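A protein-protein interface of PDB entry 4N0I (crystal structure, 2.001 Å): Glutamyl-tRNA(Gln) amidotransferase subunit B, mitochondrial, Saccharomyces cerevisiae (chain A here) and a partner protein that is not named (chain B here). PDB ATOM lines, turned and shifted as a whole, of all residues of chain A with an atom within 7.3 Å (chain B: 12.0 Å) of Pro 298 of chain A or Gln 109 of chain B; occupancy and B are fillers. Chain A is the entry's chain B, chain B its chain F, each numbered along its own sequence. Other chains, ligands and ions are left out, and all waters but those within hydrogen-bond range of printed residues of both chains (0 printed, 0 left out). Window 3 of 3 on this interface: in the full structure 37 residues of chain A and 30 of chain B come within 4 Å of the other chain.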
ATOM      1  N   MET A  72     -13.813  -4.987  -0.408  1.00  0.00           N
ATOM      2  CA  MET A  72     -13.262  -5.042  -1.769  1.00  0.00           C
ATOM      3  C   MET A  72     -14.226  -5.806  -2.684  1.00  0.00           C
ATOM      4  O   MET A  72     -14.484  -5.384  -3.819  1.00  0.00           O
ATOM      5  CB  MET A  72     -11.876  -5.691  -1.777  1.00  0.00           C
ATOM      6  CG  MET A  72     -10.728  -4.678  -1.850  1.00  0.00           C
ATOM      7  SD  MET A  72     -10.697  -3.839  -3.453  1.00  0.00           S
ATOM      8  CE  MET A  72      -9.332  -2.723  -3.207  1.00  0.00           C
ATOM      9  N   SER A  84      -8.148   5.619  -2.717  1.00  0.00           N
ATOM     10  CA  SER A  84      -6.713   5.362  -2.560  1.00  0.00           C
ATOM     11  C   SER A  84      -6.332   5.346  -1.074  1.00  0.00           C
ATOM     12  O   SER A  84      -5.591   4.482  -0.607  1.00  0.00           O
ATOM     13  CB  SER A  84      -5.893   6.419  -3.300  1.00  0.00           C
ATOM     14  OG  SER A  84      -6.146   7.715  -2.786  1.00  0.00           O
ATOM     15  N   ILE A  85      -6.895   6.276  -0.321  1.00  0.00           N
ATOM     16  CA  ILE A  85      -6.705   6.287   1.113  1.00  0.00           C
ATOM     17  C   ILE A  85      -8.064   6.371   1.768  1.00  0.00           C
ATOM     18  O   ILE A  85      -8.846   7.268   1.480  1.00  0.00           O
ATOM     19  CB  ILE A  85      -5.892   7.515   1.559  1.00  0.00           C
ATOM     20  CG1 ILE A  85      -4.521   7.501   0.896  1.00  0.00           C
ATOM     21  CG2 ILE A  85      -5.760   7.549   3.081  1.00  0.00           C
ATOM     22  CD1 ILE A  85      -3.737   6.249   1.201  1.00  0.00           C
ATOM     23  N   ASN A 295      -4.500   1.924   2.935  1.00  0.00           N
ATOM     24  CA  ASN A 295      -3.802   2.307   1.716  1.00  0.00           C
ATOM     25  C   ASN A 295      -3.519   1.061   0.890  1.00  0.00           C
ATOM     26  O   ASN A 295      -2.504   0.391   1.084  1.00  0.00           O
ATOM     27  CB  ASN A 295      -2.506   3.045   2.046  1.00  0.00           C
ATOM     28  CG  ASN A 295      -1.718   3.438   0.810  1.00  0.00           C
ATOM     29  OD1 ASN A 295      -2.259   3.536  -0.302  1.00  0.00           O
ATOM     30  ND2 ASN A 295      -0.426   3.681   0.999  1.00  0.00           N
ATOM     31  N   LEU A 296      -4.446   0.730  -0.005  1.00  0.00           N
ATOM     32  CA  LEU A 296      -4.366  -0.517  -0.749  1.00  0.00           C
ATOM     33  C   LEU A 296      -3.553  -0.354  -2.036  1.00  0.00           C
ATOM     34  O   LEU A 296      -3.699   0.628  -2.767  1.00  0.00           O
ATOM     35  CB  LEU A 296      -5.770  -1.024  -1.066  1.00  0.00           C
ATOM     36  CG  LEU A 296      -6.652  -1.243   0.174  1.00  0.00           C
ATOM     37  CD1 LEU A 296      -8.081  -1.537  -0.234  1.00  0.00           C
ATOM     38  CD2 LEU A 296      -6.114  -2.368   1.031  1.00  0.00           C
ATOM     39  N   ALA A 297      -2.713  -1.339  -2.319  1.00  0.00           N
ATOM     40  CA  ALA A 297      -1.931  -1.344  -3.551  1.00  0.00           C
ATOM     41  C   ALA A 297      -2.824  -1.733  -4.720  1.00  0.00           C
ATOM     42  O   ALA A 297      -3.837  -2.418  -4.528  1.00  0.00           O
ATOM     43  CB  ALA A 297      -0.765  -2.324  -3.433  1.00  0.00           C
ATOM     44  N   PRO A 298      -2.479  -1.262  -5.930  1.00  0.00           N
ATOM     45  CA  PRO A 298      -3.275  -1.602  -7.107  1.00  0.00           C
ATOM     46  C   PRO A 298      -3.535  -3.105  -7.283  1.00  0.00           C
ATOM     47  O   PRO A 298      -4.614  -3.462  -7.757  1.00  0.00           O
ATOM     48  CB  PRO A 298      -2.424  -1.066  -8.270  1.00  0.00           C
ATOM     49  CG  PRO A 298      -1.651   0.055  -7.680  1.00  0.00           C
ATOM     50  CD  PRO A 298      -1.338  -0.383  -6.271  1.00  0.00           C
ATOM     51  N   ASP A 299      -2.624  -3.968  -6.837  1.00  0.00           N
ATOM     52  CA  ASP A 299      -2.798  -5.407  -7.068  1.00  0.00           C
ATOM     53  C   ASP A 299      -3.865  -6.043  -6.176  1.00  0.00           C
ATOM     54  O   ASP A 299      -4.273  -7.175  -6.403  1.00  0.00           O
ATOM     55  CB  ASP A 299      -1.467  -6.176  -6.965  1.00  0.00           C
ATOM     56  CG  ASP A 299      -0.899  -6.217  -5.558  1.00  0.00           C
ATOM     57  OD1 ASP A 299      -1.585  -5.812  -4.597  1.00  0.00           O
ATOM     58  OD2 ASP A 299       0.258  -6.675  -5.411  1.00  0.00           O
ATOM     59  N   VAL A 300      -4.368  -5.291  -5.211  1.00  0.00           N
ATOM     60  CA  VAL A 300      -5.472  -5.792  -4.400  1.00  0.00           C
ATOM     61  C   VAL A 300      -6.717  -5.861  -5.264  1.00  0.00           C
ATOM     62  O   VAL A 300      -7.521  -6.786  -5.137  1.00  0.00           O
ATOM     63  CB  VAL A 300      -5.724  -4.916  -3.169  1.00  0.00           C
ATOM     64  CG1 VAL A 300      -6.946  -5.439  -2.389  1.00  0.00           C
ATOM     65  CG2 VAL A 300      -4.482  -4.904  -2.301  1.00  0.00           C
ATOM     66  N   ILE A 301      -6.873  -4.872  -6.132  1.00  0.00           N
ATOM     67  CA  ILE A 301      -7.990  -4.850  -7.066  1.00  0.00           C
ATOM     68  C   ILE A 301      -7.997  -6.067  -7.989  1.00  0.00           C
ATOM     69  O   ILE A 301      -9.000  -6.778  -8.066  1.00  0.00           O
ATOM     70  CB  ILE A 301      -7.962  -3.605  -7.939  1.00  0.00           C
ATOM     71  CG1 ILE A 301      -7.735  -2.360  -7.076  1.00  0.00           C
ATOM     72  CG2 ILE A 301      -9.237  -3.505  -8.761  1.00  0.00           C
ATOM     73  CD1 ILE A 301      -8.997  -1.779  -6.519  1.00  0.00           C
ATOM     74  N   SER A 302      -6.900  -6.309  -8.710  1.00  0.00           N
ATOM     75  CA  SER A 302      -6.867  -7.476  -9.603  1.00  0.00           C
ATOM     76  C   SER A 302      -6.910  -8.791  -8.812  1.00  0.00           C
ATOM     77  O   SER A 302      -7.522  -9.758  -9.260  1.00  0.00           O
ATOM     78  CB  SER A 302      -5.644  -7.438 -10.541  1.00  0.00           C
ATOM     79  OG  SER A 302      -4.428  -7.620  -9.847  1.00  0.00           O
ATOM     80  N   GLY A 303      -6.269  -8.823  -7.648  1.00  0.00           N
ATOM     81  CA  GLY A 303      -6.258 -10.011  -6.806  1.00  0.00           C
ATOM     82  C   GLY A 303      -7.644 -10.435  -6.340  1.00  0.00           C
ATOM     83  O   GLY A 303      -8.058 -11.582  -6.508  1.00  0.00           O
ATOM     84  N   THR B 107       3.573   5.923   3.805  1.00  0.00           N
ATOM     85  CA  THR B 107       2.762   4.791   4.242  1.00  0.00           C
ATOM     86  C   THR B 107       2.895   3.599   3.295  1.00  0.00           C
ATOM     87  O   THR B 107       2.724   3.728   2.079  1.00  0.00           O
ATOM     88  CB  THR B 107       1.266   5.171   4.351  1.00  0.00           C
ATOM     89  N   LYS B 108       3.197   2.438   3.863  1.00  0.00           N
ATOM     90  CA  LYS B 108       3.340   1.215   3.085  1.00  0.00           C
ATOM     91  C   LYS B 108       1.993   0.736   2.512  1.00  0.00           C
ATOM     92  O   LYS B 108       1.020   0.549   3.251  1.00  0.00           O
ATOM     93  CB  LYS B 108       3.974   0.120   3.950  1.00  0.00           C
ATOM     94  N   GLN B 109       1.939   0.552   1.197  1.00  0.00           N
ATOM     95  CA  GLN B 109       0.729   0.047   0.557  1.00  0.00           C
ATOM     96  C   GLN B 109       0.524  -1.424   0.878  1.00  0.00           C
ATOM     97  O   GLN B 109       1.344  -2.265   0.506  1.00  0.00           O
ATOM     98  CB  GLN B 109       0.775   0.242  -0.961  1.00  0.00           C
ATOM     99  CG  GLN B 109       0.118   1.520  -1.436  1.00  0.00           C
ATOM    100  CD  GLN B 109       0.161   1.679  -2.946  1.00  0.00           C
ATOM    101  OE1 GLN B 109       0.979   1.055  -3.626  1.00  0.00           O
ATOM    102  NE2 GLN B 109      -0.726   2.514  -3.478  1.00  0.00           N
ATOM    103  N   LEU B 110      -0.561  -1.730   1.581  1.00  0.00           N
ATOM    104  CA  LEU B 110      -0.947  -3.115   1.786  1.00  0.00           C
ATOM    105  C   LEU B 110      -1.230  -3.724   0.421  1.00  0.00           C
ATOM    106  O   LEU B 110      -2.114  -3.258  -0.299  1.00  0.00           O
ATOM    107  CB  LEU B 110      -2.201  -3.208   2.669  1.00  0.00           C
ATOM    108  CG  LEU B 110      -2.723  -4.625   2.910  1.00  0.00           C
ATOM    109  CD1 LEU B 110      -1.755  -5.405   3.775  1.00  0.00           C
ATOM    110  CD2 LEU B 110      -4.096  -4.596   3.530  1.00  0.00           C
ATOM    111  N   ASN B 111      -0.470  -4.751   0.061  1.00  0.00           N
ATOM    112  CA  ASN B 111      -0.703  -5.449  -1.195  1.00  0.00           C
ATOM    113  C   ASN B 111      -1.515  -6.712  -0.994  1.00  0.00           C
ATOM    114  O   ASN B 111      -1.761  -7.122   0.140  1.00  0.00           O
ATOM    115  CB  ASN B 111       0.608  -5.754  -1.946  1.00  0.00           C
ATOM    116  CG  ASN B 111       1.571  -6.623  -1.146  1.00  0.00           C
ATOM    117  OD1 ASN B 111       2.716  -6.238  -0.922  1.00  0.00           O
ATOM    118  ND2 ASN B 111       1.119  -7.802  -0.730  1.00  0.00           N
ATOM    119  N   TYR B 112      -1.887  -7.337  -2.103  1.00  0.00           N
ATOM    120  CA  TYR B 112      -2.757  -8.500  -2.097  1.00  0.00           C
ATOM    121  C   TYR B 112      -2.236  -9.674  -1.269  1.00  0.00           C
ATOM    122  O   TYR B 112      -2.987 -10.244  -0.482  1.00  0.00           O
ATOM    123  CB  TYR B 112      -3.065  -8.952  -3.529  1.00  0.00           C
ATOM    124  CG  TYR B 112      -4.051 -10.093  -3.590  1.00  0.00           C
ATOM    125  CD1 TYR B 112      -5.365  -9.917  -3.181  1.00  0.00           C
ATOM    126  CD2 TYR B 112      -3.669 -11.344  -4.058  1.00  0.00           C
ATOM    127  CE1 TYR B 112      -6.274 -10.955  -3.227  1.00  0.00           C
ATOM    128  CE2 TYR B 112      -4.570 -12.387  -4.115  1.00  0.00           C
ATOM    129  CZ  TYR B 112      -5.873 -12.188  -3.696  1.00  0.00           C
ATOM    130  OH  TYR B 112      -6.774 -13.224  -3.742  1.00  0.00           O
ATOM    131  N   THR B 113      -0.968 -10.041  -1.441  1.00  0.00           N
ATOM    132  CA  THR B 113      -0.426 -11.183  -0.698  1.00  0.00           C
ATOM    133  C   THR B 113      -0.376 -10.888   0.803  1.00  0.00           C
ATOM    134  O   THR B 113      -0.716 -11.744   1.623  1.00  0.00           O
ATOM    135  CB  THR B 113       0.964 -11.656  -1.223  1.00  0.00           C
ATOM    136  OG1 THR B 113       1.960 -10.657  -0.971  1.00  0.00           O
ATOM    137  CG2 THR B 113       0.907 -11.950  -2.716  1.00  0.00           C
ATOM    138  N   LYS B 114       0.025  -9.669   1.151  1.00  0.00           N
ATOM    139  CA  LYS B 114       0.037  -9.231   2.542  1.00  0.00           C
ATOM    140  C   LYS B 114      -1.373  -9.158   3.120  1.00  0.00           C
ATOM    141  O   LYS B 114      -1.581  -9.440   4.297  1.00  0.00           O
ATOM    142  CB  LYS B 114       0.747  -7.884   2.680  1.00  0.00           C
ATOM    143  CG  LYS B 114       2.233  -7.942   2.343  1.00  0.00           C
ATOM    144  CD  LYS B 114       2.936  -9.005   3.180  1.00  0.00           C
ATOM    145  CE  LYS B 114       4.395  -9.175   2.769  1.00  0.00           C
ATOM    146  NZ  LYS B 114       5.104 -10.194   3.601  1.00  0.00           N
ATOM    147  N   LEU B 115      -2.338  -8.772   2.285  1.00  0.00           N
ATOM    148  CA  LEU B 115      -3.737  -8.780   2.688  1.00  0.00           C
ATOM    149  C   LEU B 115      -4.107 -10.198   3.113  1.00  0.00           C
ATOM    150  O   LEU B 115      -4.512 -10.435   4.252  1.00  0.00           O
ATOM    151  CB  LEU B 115      -4.629  -8.324   1.533  1.00  0.00           C
ATOM    152  CG  LEU B 115      -5.985  -7.663   1.815  1.00  0.00           C
ATOM    153  CD1 LEU B 115      -7.028  -8.111   0.808  1.00  0.00           C
ATOM    154  CD2 LEU B 115      -6.480  -7.861   3.249  1.00  0.00           C
ATOM    155  N   LEU B 116      -3.934 -11.144   2.198  1.00  0.00           N
ATOM    156  CA  LEU B 116      -4.268 -12.537   2.467  1.00  0.00           C
ATOM    157  C   LEU B 116      -3.473 -13.118   3.631  1.00  0.00           C
ATOM    158  O   LEU B 116      -4.010 -13.876   4.439  1.00  0.00           O
ATOM    159  CB  LEU B 116      -4.067 -13.381   1.208  1.00  0.00           C
ATOM    160  CG  LEU B 116      -5.319 -13.617   0.362  1.00  0.00           C
ATOM    161  CD1 LEU B 116      -6.059 -12.329   0.060  1.00  0.00           C
ATOM    162  CD2 LEU B 116      -4.954 -14.338  -0.932  1.00  0.00           C
ATOM    163  N   GLU B 117      -2.199 -12.751   3.718  1.00  0.00           N
ATOM    164  CA  GLU B 117      -1.329 -13.268   4.766  1.00  0.00           C
ATOM    165  C   GLU B 117      -1.793 -12.800   6.135  1.00  0.00           C
ATOM    166  O   GLU B 117      -1.842 -13.585   7.081  1.00  0.00           O
ATOM    167  CB  GLU B 117       0.116 -12.834   4.533  1.00  0.00           C
ATOM    168  CG  GLU B 117       1.104 -13.389   5.542  1.00  0.00           C
ATOM    169  CD  GLU B 117       2.546 -13.028   5.212  1.00  0.00           C
ATOM    170  OE1 GLU B 117       2.769 -12.269   4.241  1.00  0.00           O
ATOM    171  OE2 GLU B 117       3.458 -13.507   5.922  1.00  0.00           O
ATOM    172  N   GLY B 118      -2.127 -11.516   6.234  1.00  0.00           N
ATOM    173  CA  GLY B 118      -2.603 -10.949   7.484  1.00  0.00           C
ATOM    174  C   GLY B 118      -3.873 -11.626   7.952  1.00  0.00           C
ATOM    175  O   GLY B 118      -4.038 -11.914   9.134  1.00  0.00           O
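The side-chain amide nitrogen (ND2) of Asn 295 of chain A sits at hydrogen-bond distance from the backbone carbonyl oxygen (O) of Thr 107 of chain B, 3.3 Å away.
The side-chain carboxylate of Asp 299 of chain A lies within hydrogen-bond range of the backbone NH of Tyr 112 of chain B (2.9 Å).
The backbone carbonyl oxygen (O) of Gly 303 of chain A is in hydrogen-bond range of the side-chain hydroxyl (OH) of Tyr 112 of chain B.
N of Leu 110 of chain B is in hydrogen-bond range of O of Asn 295 of chain A (2.9 Å).
N of Ala 297 of chain A is in hydrogen-bond range of O of Leu 110 of chain B (2.8 Å).
Of the 12 printed residues of chain A, 7 touch a printed residue of chain B.
Of the 12 printed residues of chain B, 5 touch a printed residue of chain A.
Printed residues of chain B that touch a printed residue of chain A: Thr 107, Gln 109, Leu 110, Asn 111 and Tyr 112.
Hydrophobic or aromatic side chains of chain B within 4 Å of the printed part of chain A: Leu 110 and Tyr 112.
Among the printed residues, 15 pairs touch across the chains.
Among the printed residues, no Asp or Glu carboxylate lies within 4 Å of a Lys or Arg side-chain nitrogen of the other chain.
Pro 298 of chain A touches just one residue of chain B: Gln 109 (3.8 Å).
Gln 109 of chain B touches four residues of chain A.
Of chain B, only Thr 107, Gln 109 and Leu 110 come within 4 Å of Asn 295 of chain A.
Of chain B, only Gln 109 (3.7 Å), Leu 110 (2.8 Å) and Asn 111 (3.8 Å) come within 4 Å of Ala 297 of chain A.
Of chain B, only Asn 111 and Tyr 112 come within 4 Å of Asp 299 of chain A.
Val 300 of chain A touches three residues of chain B.
Of the printed residues of chain A, Tyr 112 of chain B touches Asp 299 (2.9 Å), Val 300 (3.6 Å) and Gly 303 (3.4 Å).
Printed residues of chain B within 4 Å of Gly 303 of chain A: Tyr 112.
Ile 85 of chain A touches none of the printed residues of chain B.
Thr 113 of chain B touches none of the printed residues of chain A.
The nearest printed residue of chain A that does not touch Tyr 112 of chain B is Ala 297 of chain A (5.3 Å).
The side-chain amide nitrogen (ND2) of Asn 111 of chain B sits close to the backbone NH (N) of Lys 114 of chain B (2.9 Å).
The backbone carbonyl oxygen (O) of Ser 84 of chain A lies close to the side-chain amide oxygen (OD1) of Asn 295 of chain A (3.5 Å).
OG1 of Thr 113 of chain B sits at hydrogen-bond distance from ND2 of Asn 111 of chain B, 3.0 Å away.
The backbone carbonyl oxygen of Asp 299 of chain A sits at hydrogen-bond distance from the side-chain hydroxyl of Ser 302 of chain A, 3.5 Å away.
Among the printed residues, pairs that only touch across the chains: Asn 295 of chain A with Gln 109 of chain B, Asp 299 of chain A with Asn 111 of chain B, Val 300 of chain A with Leu 110 of chain B, Val 300 of chain A with Tyr 112 of chain B, Leu 296 of chain A with Leu 110 of chain B, Leu 296 of chain A with Gln 109 of chain B, Val 300 of chain A with Asn 111 of chain B, Ala 297 of chain A with Gln 109 of chain B, Pro 298 of chain A with Gln 109 of chain B and Ala 297 of chain A with Asn 111 of chain B.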
